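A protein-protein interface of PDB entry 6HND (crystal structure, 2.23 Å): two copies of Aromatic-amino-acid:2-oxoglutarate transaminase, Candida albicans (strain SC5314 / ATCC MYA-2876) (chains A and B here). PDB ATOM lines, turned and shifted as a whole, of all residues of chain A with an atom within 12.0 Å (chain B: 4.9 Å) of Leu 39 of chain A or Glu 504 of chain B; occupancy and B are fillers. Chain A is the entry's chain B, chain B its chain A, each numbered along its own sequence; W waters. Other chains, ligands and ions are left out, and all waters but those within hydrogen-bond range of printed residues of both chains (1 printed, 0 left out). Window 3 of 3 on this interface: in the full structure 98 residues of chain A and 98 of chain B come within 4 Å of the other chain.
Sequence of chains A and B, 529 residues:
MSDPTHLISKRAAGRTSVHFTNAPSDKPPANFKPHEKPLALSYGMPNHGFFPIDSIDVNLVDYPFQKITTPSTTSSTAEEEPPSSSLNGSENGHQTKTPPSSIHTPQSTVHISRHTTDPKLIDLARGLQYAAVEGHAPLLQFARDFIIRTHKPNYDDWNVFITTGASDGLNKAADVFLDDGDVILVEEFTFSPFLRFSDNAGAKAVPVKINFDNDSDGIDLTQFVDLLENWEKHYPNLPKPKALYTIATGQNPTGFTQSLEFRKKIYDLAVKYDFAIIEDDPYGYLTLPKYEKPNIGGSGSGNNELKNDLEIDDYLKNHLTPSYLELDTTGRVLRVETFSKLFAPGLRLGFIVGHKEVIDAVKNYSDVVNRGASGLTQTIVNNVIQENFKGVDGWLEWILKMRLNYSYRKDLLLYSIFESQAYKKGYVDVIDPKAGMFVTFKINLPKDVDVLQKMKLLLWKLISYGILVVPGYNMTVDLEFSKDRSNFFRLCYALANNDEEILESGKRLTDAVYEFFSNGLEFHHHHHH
The backbone NH (N) of Leu 468 of chain B sits at hydrogen-bond distance from the backbone carbonyl oxygen (O) of Leu 39 of chain A, 3.0 Å away.
O of Lys 37 of chain A is in hydrogen-bond range of NH1 of Arg 508 of chain B (3.1 Å).
The backbone NH (N) of Leu 41 of chain A sits at hydrogen-bond distance from the backbone carbonyl oxygen (O) of Leu 468 of chain B (2.6 Å).
O of Leu 468 of chain B lies within hydrogen-bond range of N of Ser 42 of chain A (3.1 Å).
N of Leu 39 of chain A is in hydrogen-bond range of O of Gly 466 of chain B (2.9 Å).
The backbone carbonyl oxygen (O) of Gly 466 of chain B lies within hydrogen-bond range of the guanidinium group (NH1) of Arg 508 of chain B, 3.0 Å away.
The backbone carbonyl oxygen of Glu 501 of chain B lies within hydrogen-bond range of the side-chain hydroxyl of Ser 505 of chain B, at 2.5 Å.
N of Lys 37 of chain A is in hydrogen-bond range of ND1 of His 35 of chain A (3.2 Å).
OE2 of Glu 504 of chain B is in salt-bridge range of NE of Arg 508 of chain B.
His 35 of chain A touches Gly 466 of chain B (CB to CA, 3.4 Å).
His 35 of chain A touches Arg 508 of chain B.
Pro 38 of chain A touches Gly 466 of chain B.
O of Leu 39 of chain A touches CA of Ile 467 of chain B, at 3.3 Å.
Leu 39 of chain A touches Glu 501 of chain B (CD2 to CG, 3.8 Å).
CD1 of Leu 39 of chain A touches CG of Glu 504 of chain B, 3.6 Å away.
CB of Leu 39 of chain A touches OG of Ser 505 of chain B, at 3.7 Å.
Leu 39 of chain A touches Arg 508 of chain B (N to NH1, 3.8 Å).
Ala 40 of chain A touches Leu 468 of chain B (C to O, 3.6 Å).
Ile 467 of chain B touches Leu 41 of chain A (CD1 to CD1, 3.8 Å).
Printed residues of chain B within 4 Å of His 35 of chain A: Gly 466 (3.4 Å) and Arg 508 (3.7 Å).
Of the printed residues of chain B, Pro 38 of chain A touches Gly 466 (3.5 Å).
Leu 39 of chain A touches seven residues of chain B.
Printed residues of chain B within 4 Å of Leu 41 of chain A: Ile 467, Leu 468 and Ser 505.
Of the printed residues of chain B, Ser 42 of chain A touches Leu 468 (3.1 Å).
Of chain A, only Leu 39 and Leu 41 come within 4 Å of Ile 467 of chain B.
Glu 501 of chain B touches just one residue of chain A: Leu 39.
Of chain A, only Leu 39 (3.7 Å) and Leu 41 (3.7 Å) come within 4 Å of Ser 505 of chain B.
Gly 506 of chain B touches none of the printed residues of chain A.
No residue of chain A comes within 4 Å of Lys 507 of chain B.
Of chain A, only His 35, Lys 37 and Leu 39 come within 4 Å of Arg 508 of chain B.
The nearest printed residue of chain B that does not touch Leu 39 of chain A is Glu 500 of chain B (5.6 Å).
The nearest residue of chain A that does not touch Glu 504 of chain B is His 35 of chain A (6.5 Å).
The nearest printed residue of chain B that does not touch Pro 38 of chain A is Arg 508 of chain B (4.1 Å).
Of the 15 printed residues of chain A, 7 touch a printed residue of chain B.
Hydrophobic or aromatic side chains of chain A within 4 Å of the printed part of chain B: His 35, Pro 38, Leu 39 and Leu 41.
Printed residues of chain B that touch a printed residue of chain A: Gly 466, Ile 467, Leu 468, Glu 501, Glu 504, Ser 505 and Arg 508.
Hydrophobic or aromatic side chains of chain B that line the printed part of chain A: Ile 467 and Leu 468.
Among the printed residues, no Asp or Glu carboxylate lies within 4 Å of a Lys or Arg side-chain nitrogen of the other chain.
No position is printed for both chains.
Water W1 lies within hydrogen-bond range of NH2 of Arg 508 of chain B (2.7 Å) and O of Lys 37 of chain A (3.0 Å).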
ATOM      1  N   PHE A  32      16.561 -25.621 -26.381  1.00  0.00           N
ATOM      2  CA  PHE A  32      15.598 -25.860 -25.277  1.00  0.00           C
ATOM      3  C   PHE A  32      15.195 -27.338 -25.249  1.00  0.00           C
ATOM      4  O   PHE A  32      14.784 -27.883 -26.282  1.00  0.00           O
ATOM      5  CB  PHE A  32      14.364 -24.967 -25.382  1.00  0.00           C
ATOM      6  CG  PHE A  32      13.247 -25.425 -24.488  1.00  0.00           C
ATOM      7  CD1 PHE A  32      13.303 -25.199 -23.124  1.00  0.00           C
ATOM      8  CD2 PHE A  32      12.157 -26.112 -25.005  1.00  0.00           C
ATOM      9  CE1 PHE A  32      12.276 -25.622 -22.298  1.00  0.00           C
ATOM     10  CE2 PHE A  32      11.129 -26.532 -24.171  1.00  0.00           C
ATOM     11  CZ  PHE A  32      11.195 -26.287 -22.818  1.00  0.00           C
ATOM     12  N   LYS A  33      15.340 -27.956 -24.078  1.00  0.00           N
ATOM     13  CA  LYS A  33      14.883 -29.327 -23.762  1.00  0.00           C
ATOM     14  C   LYS A  33      14.107 -29.235 -22.454  1.00  0.00           C
ATOM     15  O   LYS A  33      14.646 -28.787 -21.440  1.00  0.00           O
ATOM     16  CB  LYS A  33      16.094 -30.265 -23.664  1.00  0.00           C
ATOM     17  CG  LYS A  33      15.788 -31.756 -23.539  1.00  0.00           C
ATOM     18  CD  LYS A  33      17.041 -32.624 -23.358  1.00  0.00           C
ATOM     19  CE  LYS A  33      16.776 -34.115 -23.471  1.00  0.00           C
ATOM     20  NZ  LYS A  33      15.850 -34.596 -22.415  1.00  0.00           N
ATOM     21  N   PRO A  34      12.823 -29.655 -22.427  1.00  0.00           N
ATOM     22  CA  PRO A  34      12.048 -29.644 -21.193  1.00  0.00           C
ATOM     23  C   PRO A  34      12.691 -30.640 -20.227  1.00  0.00           C
ATOM     24  O   PRO A  34      13.269 -31.587 -20.689  1.00  0.00           O
ATOM     25  CB  PRO A  34      10.648 -30.114 -21.607  1.00  0.00           C
ATOM     26  CG  PRO A  34      10.891 -30.922 -22.865  1.00  0.00           C
ATOM     27  CD  PRO A  34      12.080 -30.262 -23.540  1.00  0.00           C
ATOM     28  N   HIS A  35      12.606 -30.373 -18.928  1.00  0.00           N
ATOM     29  CA  HIS A  35      13.173 -31.238 -17.867  1.00  0.00           C
ATOM     30  C   HIS A  35      12.203 -32.409 -17.713  1.00  0.00           C
ATOM     31  O   HIS A  35      10.989 -32.170 -17.909  1.00  0.00           O
ATOM     32  CB  HIS A  35      13.402 -30.387 -16.619  1.00  0.00           C
ATOM     33  CG  HIS A  35      14.071 -31.081 -15.484  1.00  0.00           C
ATOM     34  ND1 HIS A  35      13.504 -32.160 -14.837  1.00  0.00           N
ATOM     35  CD2 HIS A  35      15.208 -30.800 -14.823  1.00  0.00           C
ATOM     36  CE1 HIS A  35      14.303 -32.557 -13.868  1.00  0.00           C
ATOM     37  NE2 HIS A  35      15.347 -31.732 -13.825  1.00  0.00           N
ATOM     38  N   GLU A  36      12.707 -33.610 -17.401  1.00  0.00           N
ATOM     39  CA  GLU A  36      11.916 -34.875 -17.448  1.00  0.00           C
ATOM     40  C   GLU A  36      10.971 -34.981 -16.235  1.00  0.00           C
ATOM     41  O   GLU A  36       9.849 -35.521 -16.403  1.00  0.00           O
ATOM     42  CB  GLU A  36      12.863 -36.077 -17.605  1.00  0.00           C
ATOM     43  CG  GLU A  36      13.418 -36.263 -19.029  1.00  0.00           C
ATOM     44  CD  GLU A  36      12.394 -36.586 -20.119  1.00  0.00           C
ATOM     45  OE1 GLU A  36      11.734 -37.643 -20.026  1.00  0.00           O
ATOM     46  OE2 GLU A  36      12.227 -35.770 -21.052  1.00  0.00           O
ATOM     47  N   LYS A  37      11.383 -34.490 -15.056  1.00  0.00           N
ATOM     48  CA  LYS A  37      10.535 -34.397 -13.829  1.00  0.00           C
ATOM     49  C   LYS A  37      10.567 -32.971 -13.278  1.00  0.00           C
ATOM     50  O   LYS A  37      11.307 -32.674 -12.328  1.00  0.00           O
ATOM     51  CB  LYS A  37      11.021 -35.386 -12.769  1.00  0.00           C
ATOM     52  CG  LYS A  37      11.437 -36.728 -13.334  1.00  0.00           C
ATOM     53  CD  LYS A  37      11.370 -37.845 -12.353  1.00  0.00           C
ATOM     54  CE  LYS A  37      11.092 -39.168 -13.031  1.00  0.00           C
ATOM     55  NZ  LYS A  37      11.032 -40.234 -12.016  1.00  0.00           N
ATOM     56  N   PRO A  38       9.758 -32.046 -13.852  1.00  0.00           N
ATOM     57  CA  PRO A  38       9.693 -30.674 -13.351  1.00  0.00           C
ATOM     58  C   PRO A  38       8.966 -30.641 -12.004  1.00  0.00           C
ATOM     59  O   PRO A  38       8.111 -31.475 -11.790  1.00  0.00           O
ATOM     60  CB  PRO A  38       8.928 -29.917 -14.452  1.00  0.00           C
ATOM     61  CG  PRO A  38       8.058 -30.982 -15.085  1.00  0.00           C
ATOM     62  CD  PRO A  38       8.855 -32.272 -14.990  1.00  0.00           C
ATOM     63  N   LEU A  39       9.357 -29.723 -11.117  1.00  0.00           N
ATOM     64  CA  LEU A  39       8.530 -29.306  -9.943  1.00  0.00           C
ATOM     65  C   LEU A  39       7.748 -28.038 -10.310  1.00  0.00           C
ATOM     66  O   LEU A  39       8.211 -27.272 -11.180  1.00  0.00           O
ATOM     67  CB  LEU A  39       9.422 -29.099  -8.721  1.00  0.00           C
ATOM     68  CG  LEU A  39      10.092 -30.380  -8.219  1.00  0.00           C
ATOM     69  CD1 LEU A  39      11.227 -30.067  -7.237  1.00  0.00           C
ATOM     70  CD2 LEU A  39       9.053 -31.318  -7.614  1.00  0.00           C
ATOM     71  N   ALA A  40       6.558 -27.891  -9.731  1.00  0.00           N
ATOM     72  CA  ALA A  40       5.589 -26.818 -10.041  1.00  0.00           C
ATOM     73  C   ALA A  40       5.469 -25.863  -8.849  1.00  0.00           C
ATOM     74  O   ALA A  40       5.230 -26.327  -7.731  1.00  0.00           O
ATOM     75  CB  ALA A  40       4.271 -27.463 -10.371  1.00  0.00           C
ATOM     76  N   LEU A  41       5.635 -24.569  -9.094  1.00  0.00           N
ATOM     77  CA  LEU A  41       5.215 -23.474  -8.177  1.00  0.00           C
ATOM     78  C   LEU A  41       4.136 -22.652  -8.893  1.00  0.00           C
ATOM     79  O   LEU A  41       3.945 -21.463  -8.511  1.00  0.00           O
ATOM     80  CB  LEU A  41       6.425 -22.592  -7.826  1.00  0.00           C
ATOM     81  CG  LEU A  41       7.486 -23.217  -6.928  1.00  0.00           C
ATOM     82  CD1 LEU A  41       8.694 -22.305  -6.820  1.00  0.00           C
ATOM     83  CD2 LEU A  41       6.929 -23.527  -5.545  1.00  0.00           C
ATOM     84  N   SER A  42       3.452 -23.241  -9.886  1.00  0.00           N
ATOM     85  CA  SER A  42       2.586 -22.487 -10.831  1.00  0.00           C
ATOM     86  C   SER A  42       1.149 -22.408 -10.294  1.00  0.00           C
ATOM     87  O   SER A  42       0.760 -21.341  -9.824  1.00  0.00           O
ATOM     88  CB  SER A  42       2.663 -23.049 -12.239  1.00  0.00           C
ATOM     89  OG  SER A  42       2.638 -24.456 -12.222  1.00  0.00           O
ATOM     90  N   TYR A  43       0.419 -23.510 -10.301  1.00  0.00           N
ATOM     91  CA  TYR A  43      -1.057 -23.533 -10.134  1.00  0.00           C
ATOM     92  C   TYR A  43      -1.411 -23.354  -8.649  1.00  0.00           C
ATOM     93  O   TYR A  43      -0.739 -23.964  -7.833  1.00  0.00           O
ATOM     94  CB  TYR A  43      -1.656 -24.839 -10.670  1.00  0.00           C
ATOM     95  CG  TYR A  43      -0.920 -25.571 -11.776  1.00  0.00           C
ATOM     96  CD1 TYR A  43       0.018 -26.555 -11.481  1.00  0.00           C
ATOM     97  CD2 TYR A  43      -1.228 -25.357 -13.117  1.00  0.00           C
ATOM     98  CE1 TYR A  43       0.669 -27.266 -12.479  1.00  0.00           C
ATOM     99  CE2 TYR A  43      -0.589 -26.063 -14.129  1.00  0.00           C
ATOM    100  CZ  TYR A  43       0.367 -27.018 -13.807  1.00  0.00           C
ATOM    101  OH  TYR A  43       1.014 -27.715 -14.786  1.00  0.00           O
ATOM    102  N   GLY A  44      -2.474 -22.598  -8.342  1.00  0.00           N
ATOM    103  CA  GLY A  44      -3.006 -22.341  -6.988  1.00  0.00           C
ATOM    104  C   GLY A  44      -3.850 -23.485  -6.462  1.00  0.00           C
ATOM    105  O   GLY A  44      -4.981 -23.242  -6.061  1.00  0.00           O
ATOM    106  N   MET A  45      -3.315 -24.705  -6.475  1.00  0.00           N
ATOM    107  CA  MET A  45      -3.965 -25.955  -5.991  1.00  0.00           C
ATOM    108  C   MET A  45      -3.358 -26.330  -4.647  1.00  0.00           C
ATOM    109  O   MET A  45      -2.145 -26.441  -4.526  1.00  0.00           O
ATOM    110  CB  MET A  45      -3.725 -27.123  -6.949  1.00  0.00           C
ATOM    111  CG  MET A  45      -4.266 -26.877  -8.332  1.00  0.00           C
ATOM    112  SD  MET A  45      -3.804 -28.214  -9.404  1.00  0.00           S
ATOM    113  CE  MET A  45      -4.094 -27.488 -11.014  1.00  0.00           C
ATOM    114  N   ASN A  47      -2.167 -28.991  -2.245  1.00  0.00           N
ATOM    115  CA  ASN A  47      -1.839 -30.437  -2.156  1.00  0.00           C
ATOM    116  C   ASN A  47      -2.974 -31.185  -1.446  1.00  0.00           C
ATOM    117  O   ASN A  47      -3.489 -30.642  -0.482  1.00  0.00           O
ATOM    118  CB  ASN A  47      -0.534 -30.654  -1.400  1.00  0.00           C
ATOM    119  CG  ASN A  47      -0.058 -32.077  -1.543  1.00  0.00           C
ATOM    120  OD1 ASN A  47      -0.475 -32.953  -0.769  1.00  0.00           O
ATOM    121  ND2 ASN A  47       0.782 -32.312  -2.542  1.00  0.00           N
ATOM    122  N   GLY B 466      13.432 -27.257 -14.915  1.00  0.00           N
ATOM    123  CA  GLY B 466      12.471 -28.151 -14.238  1.00  0.00           C
ATOM    124  C   GLY B 466      11.785 -27.441 -13.085  1.00  0.00           C
ATOM    125  O   GLY B 466      11.605 -28.063 -12.009  1.00  0.00           O
ATOM    126  N   ILE B 467      11.439 -26.167 -13.286  1.00  0.00           N
ATOM    127  CA  ILE B 467      10.638 -25.338 -12.336  1.00  0.00           C
ATOM    128  C   ILE B 467       9.582 -24.593 -13.157  1.00  0.00           C
ATOM    129  O   ILE B 467       9.962 -23.905 -14.151  1.00  0.00           O
ATOM    130  CB  ILE B 467      11.539 -24.403 -11.493  1.00  0.00           C
ATOM    131  CG1 ILE B 467      10.760 -23.718 -10.365  1.00  0.00           C
ATOM    132  CG2 ILE B 467      12.293 -23.389 -12.333  1.00  0.00           C
ATOM    133  CD1 ILE B 467       9.953 -24.684  -9.506  1.00  0.00           C
ATOM    134  N   LEU B 468       8.310 -24.787 -12.791  1.00  0.00           N
ATOM    135  CA  LEU B 468       7.121 -24.178 -13.453  1.00  0.00           C
ATOM    136  C   LEU B 468       6.539 -23.090 -12.545  1.00  0.00           C
ATOM    137  O   LEU B 468       6.213 -23.365 -11.341  1.00  0.00           O
ATOM    138  CB  LEU B 468       6.073 -25.257 -13.740  1.00  0.00           C
ATOM    139  CG  LEU B 468       6.588 -26.492 -14.486  1.00  0.00           C
ATOM    140  CD1 LEU B 468       5.501 -27.558 -14.609  1.00  0.00           C
ATOM    141  CD2 LEU B 468       7.137 -26.122 -15.857  1.00  0.00           C
ATOM    142  N   GLU B 500      11.177 -30.806   1.135  1.00  0.00           N
ATOM    143  CA  GLU B 500      12.268 -31.104   0.172  1.00  0.00           C
ATOM    144  C   GLU B 500      11.889 -30.534  -1.200  1.00  0.00           C
ATOM    145  O   GLU B 500      12.761 -29.991  -1.873  1.00  0.00           O
ATOM    146  CB  GLU B 500      12.548 -32.609   0.108  1.00  0.00           C
ATOM    147  CG  GLU B 500      13.224 -33.173   1.353  1.00  0.00           C
ATOM    148  CD  GLU B 500      12.324 -33.396   2.558  1.00  0.00           C
ATOM    149  OE1 GLU B 500      11.146 -33.745   2.368  1.00  0.00           O
ATOM    150  OE2 GLU B 500      12.811 -33.218   3.687  1.00  0.00           O
ATOM    151  N   GLU B 501      10.627 -30.643  -1.611  1.00  0.00           N
ATOM    152  CA  GLU B 501      10.202 -30.111  -2.934  1.00  0.00           C
ATOM    153  C   GLU B 501      10.268 -28.578  -2.934  1.00  0.00           C
ATOM    154  O   GLU B 501      10.597 -28.002  -4.005  1.00  0.00           O
ATOM    155  CB  GLU B 501       8.809 -30.602  -3.313  1.00  0.00           C
ATOM    156  CG  GLU B 501       8.833 -31.990  -3.919  1.00  0.00           C
ATOM    157  CD  GLU B 501       7.458 -32.593  -4.090  1.00  0.00           C
ATOM    158  OE1 GLU B 501       6.493 -31.807  -4.229  1.00  0.00           O
ATOM    159  OE2 GLU B 501       7.368 -33.839  -4.072  1.00  0.00           O
ATOM    160  N   ILE B 502       9.981 -27.940  -1.797  1.00  0.00           N
ATOM    161  CA  ILE B 502       9.929 -26.456  -1.729  1.00  0.00           C
ATOM    162  C   ILE B 502      11.363 -25.968  -1.907  1.00  0.00           C
ATOM    163  O   ILE B 502      11.587 -25.073  -2.761  1.00  0.00           O
ATOM    164  CB  ILE B 502       9.280 -25.968  -0.419  1.00  0.00           C
ATOM    165  CG1 ILE B 502       7.868 -26.534  -0.245  1.00  0.00           C
ATOM    166  CG2 ILE B 502       9.334 -24.448  -0.312  1.00  0.00           C
ATOM    167  CD1 ILE B 502       6.759 -25.532  -0.278  1.00  0.00           C
ATOM    168  N   LEU B 503      12.298 -26.553  -1.143  1.00  0.00           N
ATOM    169  CA  LEU B 503      13.743 -26.166  -1.152  1.00  0.00           C
ATOM    170  C   LEU B 503      14.315 -26.443  -2.547  1.00  0.00           C
ATOM    171  O   LEU B 503      14.981 -25.553  -3.114  1.00  0.00           O
ATOM    172  CB  LEU B 503      14.517 -26.904  -0.049  1.00  0.00           C
ATOM    173  CG  LEU B 503      14.187 -26.493   1.390  1.00  0.00           C
ATOM    174  CD1 LEU B 503      14.803 -27.461   2.413  1.00  0.00           C
ATOM    175  CD2 LEU B 503      14.642 -25.056   1.658  1.00  0.00           C
ATOM    176  N   GLU B 504      13.999 -27.586  -3.144  1.00  0.00           N
ATOM    177  CA  GLU B 504      14.500 -27.908  -4.500  1.00  0.00           C
ATOM    178  C   GLU B 504      13.900 -26.904  -5.490  1.00  0.00           C
ATOM    179  O   GLU B 504      14.655 -26.451  -6.390  1.00  0.00           O
ATOM    180  CB  GLU B 504      14.221 -29.361  -4.872  1.00  0.00           C
ATOM    181  CG  GLU B 504      14.679 -29.727  -6.278  1.00  0.00           C
ATOM    182  CD  GLU B 504      16.175 -29.659  -6.518  1.00  0.00           C
ATOM    183  OE1 GLU B 504      16.935 -29.579  -5.496  1.00  0.00           O
ATOM    184  OE2 GLU B 504      16.593 -29.710  -7.725  1.00  0.00           O
ATOM    185  N   SER B 505      12.631 -26.516  -5.301  1.00  0.00           N
ATOM    186  CA  SER B 505      11.911 -25.562  -6.192  1.00  0.00           C
ATOM    187  C   SER B 505      12.626 -24.204  -6.233  1.00  0.00           C
ATOM    188  O   SER B 505      12.894 -23.717  -7.315  1.00  0.00           O
ATOM    189  CB  SER B 505      10.454 -25.417  -5.776  1.00  0.00           C
ATOM    190  OG  SER B 505       9.804 -26.656  -5.981  1.00  0.00           O
ATOM    191  N   GLY B 506      12.869 -23.618  -5.070  1.00  0.00           N
ATOM    192  CA  GLY B 506      13.619 -22.368  -4.925  1.00  0.00           C
ATOM    193  C   GLY B 506      15.010 -22.474  -5.498  1.00  0.00           C
ATOM    194  O   GLY B 506      15.520 -21.464  -5.991  1.00  0.00           O
ATOM    195  N   LYS B 507      15.644 -23.640  -5.393  1.00  0.00           N
ATOM    196  CA  LYS B 507      17.024 -23.854  -5.891  1.00  0.00           C
ATOM    197  C   LYS B 507      17.006 -23.798  -7.419  1.00  0.00           C
ATOM    198  O   LYS B 507      17.797 -23.026  -7.994  1.00  0.00           O
ATOM    199  CB  LYS B 507      17.583 -25.183  -5.379  1.00  0.00           C
ATOM    200  CG  LYS B 507      18.923 -25.602  -5.996  1.00  0.00           C
ATOM    201  CD  LYS B 507      19.739 -26.554  -5.132  1.00  0.00           C
ATOM    202  CE  LYS B 507      20.548 -27.575  -5.908  1.00  0.00           C
ATOM    203  NZ  LYS B 507      21.244 -26.998  -7.088  1.00  0.00           N
ATOM    204  N   ARG B 508      16.124 -24.569  -8.055  1.00  0.00           N
ATOM    205  CA  ARG B 508      16.005 -24.619  -9.532  1.00  0.00           C
ATOM    206  C   ARG B 508      15.656 -23.229 -10.073  1.00  0.00           C
ATOM    207  O   ARG B 508      16.192 -22.833 -11.137  1.00  0.00           O
ATOM    208  CB  ARG B 508      14.957 -25.643  -9.949  1.00  0.00           C
ATOM    209  CG  ARG B 508      15.402 -27.080  -9.750  1.00  0.00           C
ATOM    210  CD  ARG B 508      14.294 -28.054 -10.101  1.00  0.00           C
ATOM    211  NE  ARG B 508      14.593 -29.408  -9.641  1.00  0.00           N
ATOM    212  CZ  ARG B 508      14.016 -30.514 -10.090  1.00  0.00           C
ATOM    213  NH1 ARG B 508      13.104 -30.457 -11.044  1.00  0.00           N
ATOM    214  NH2 ARG B 508      14.359 -31.680  -9.570  1.00  0.00           N
HETATM  215  O   HOH W   1      12.871 -33.899 -10.060  1.00  0.00           O
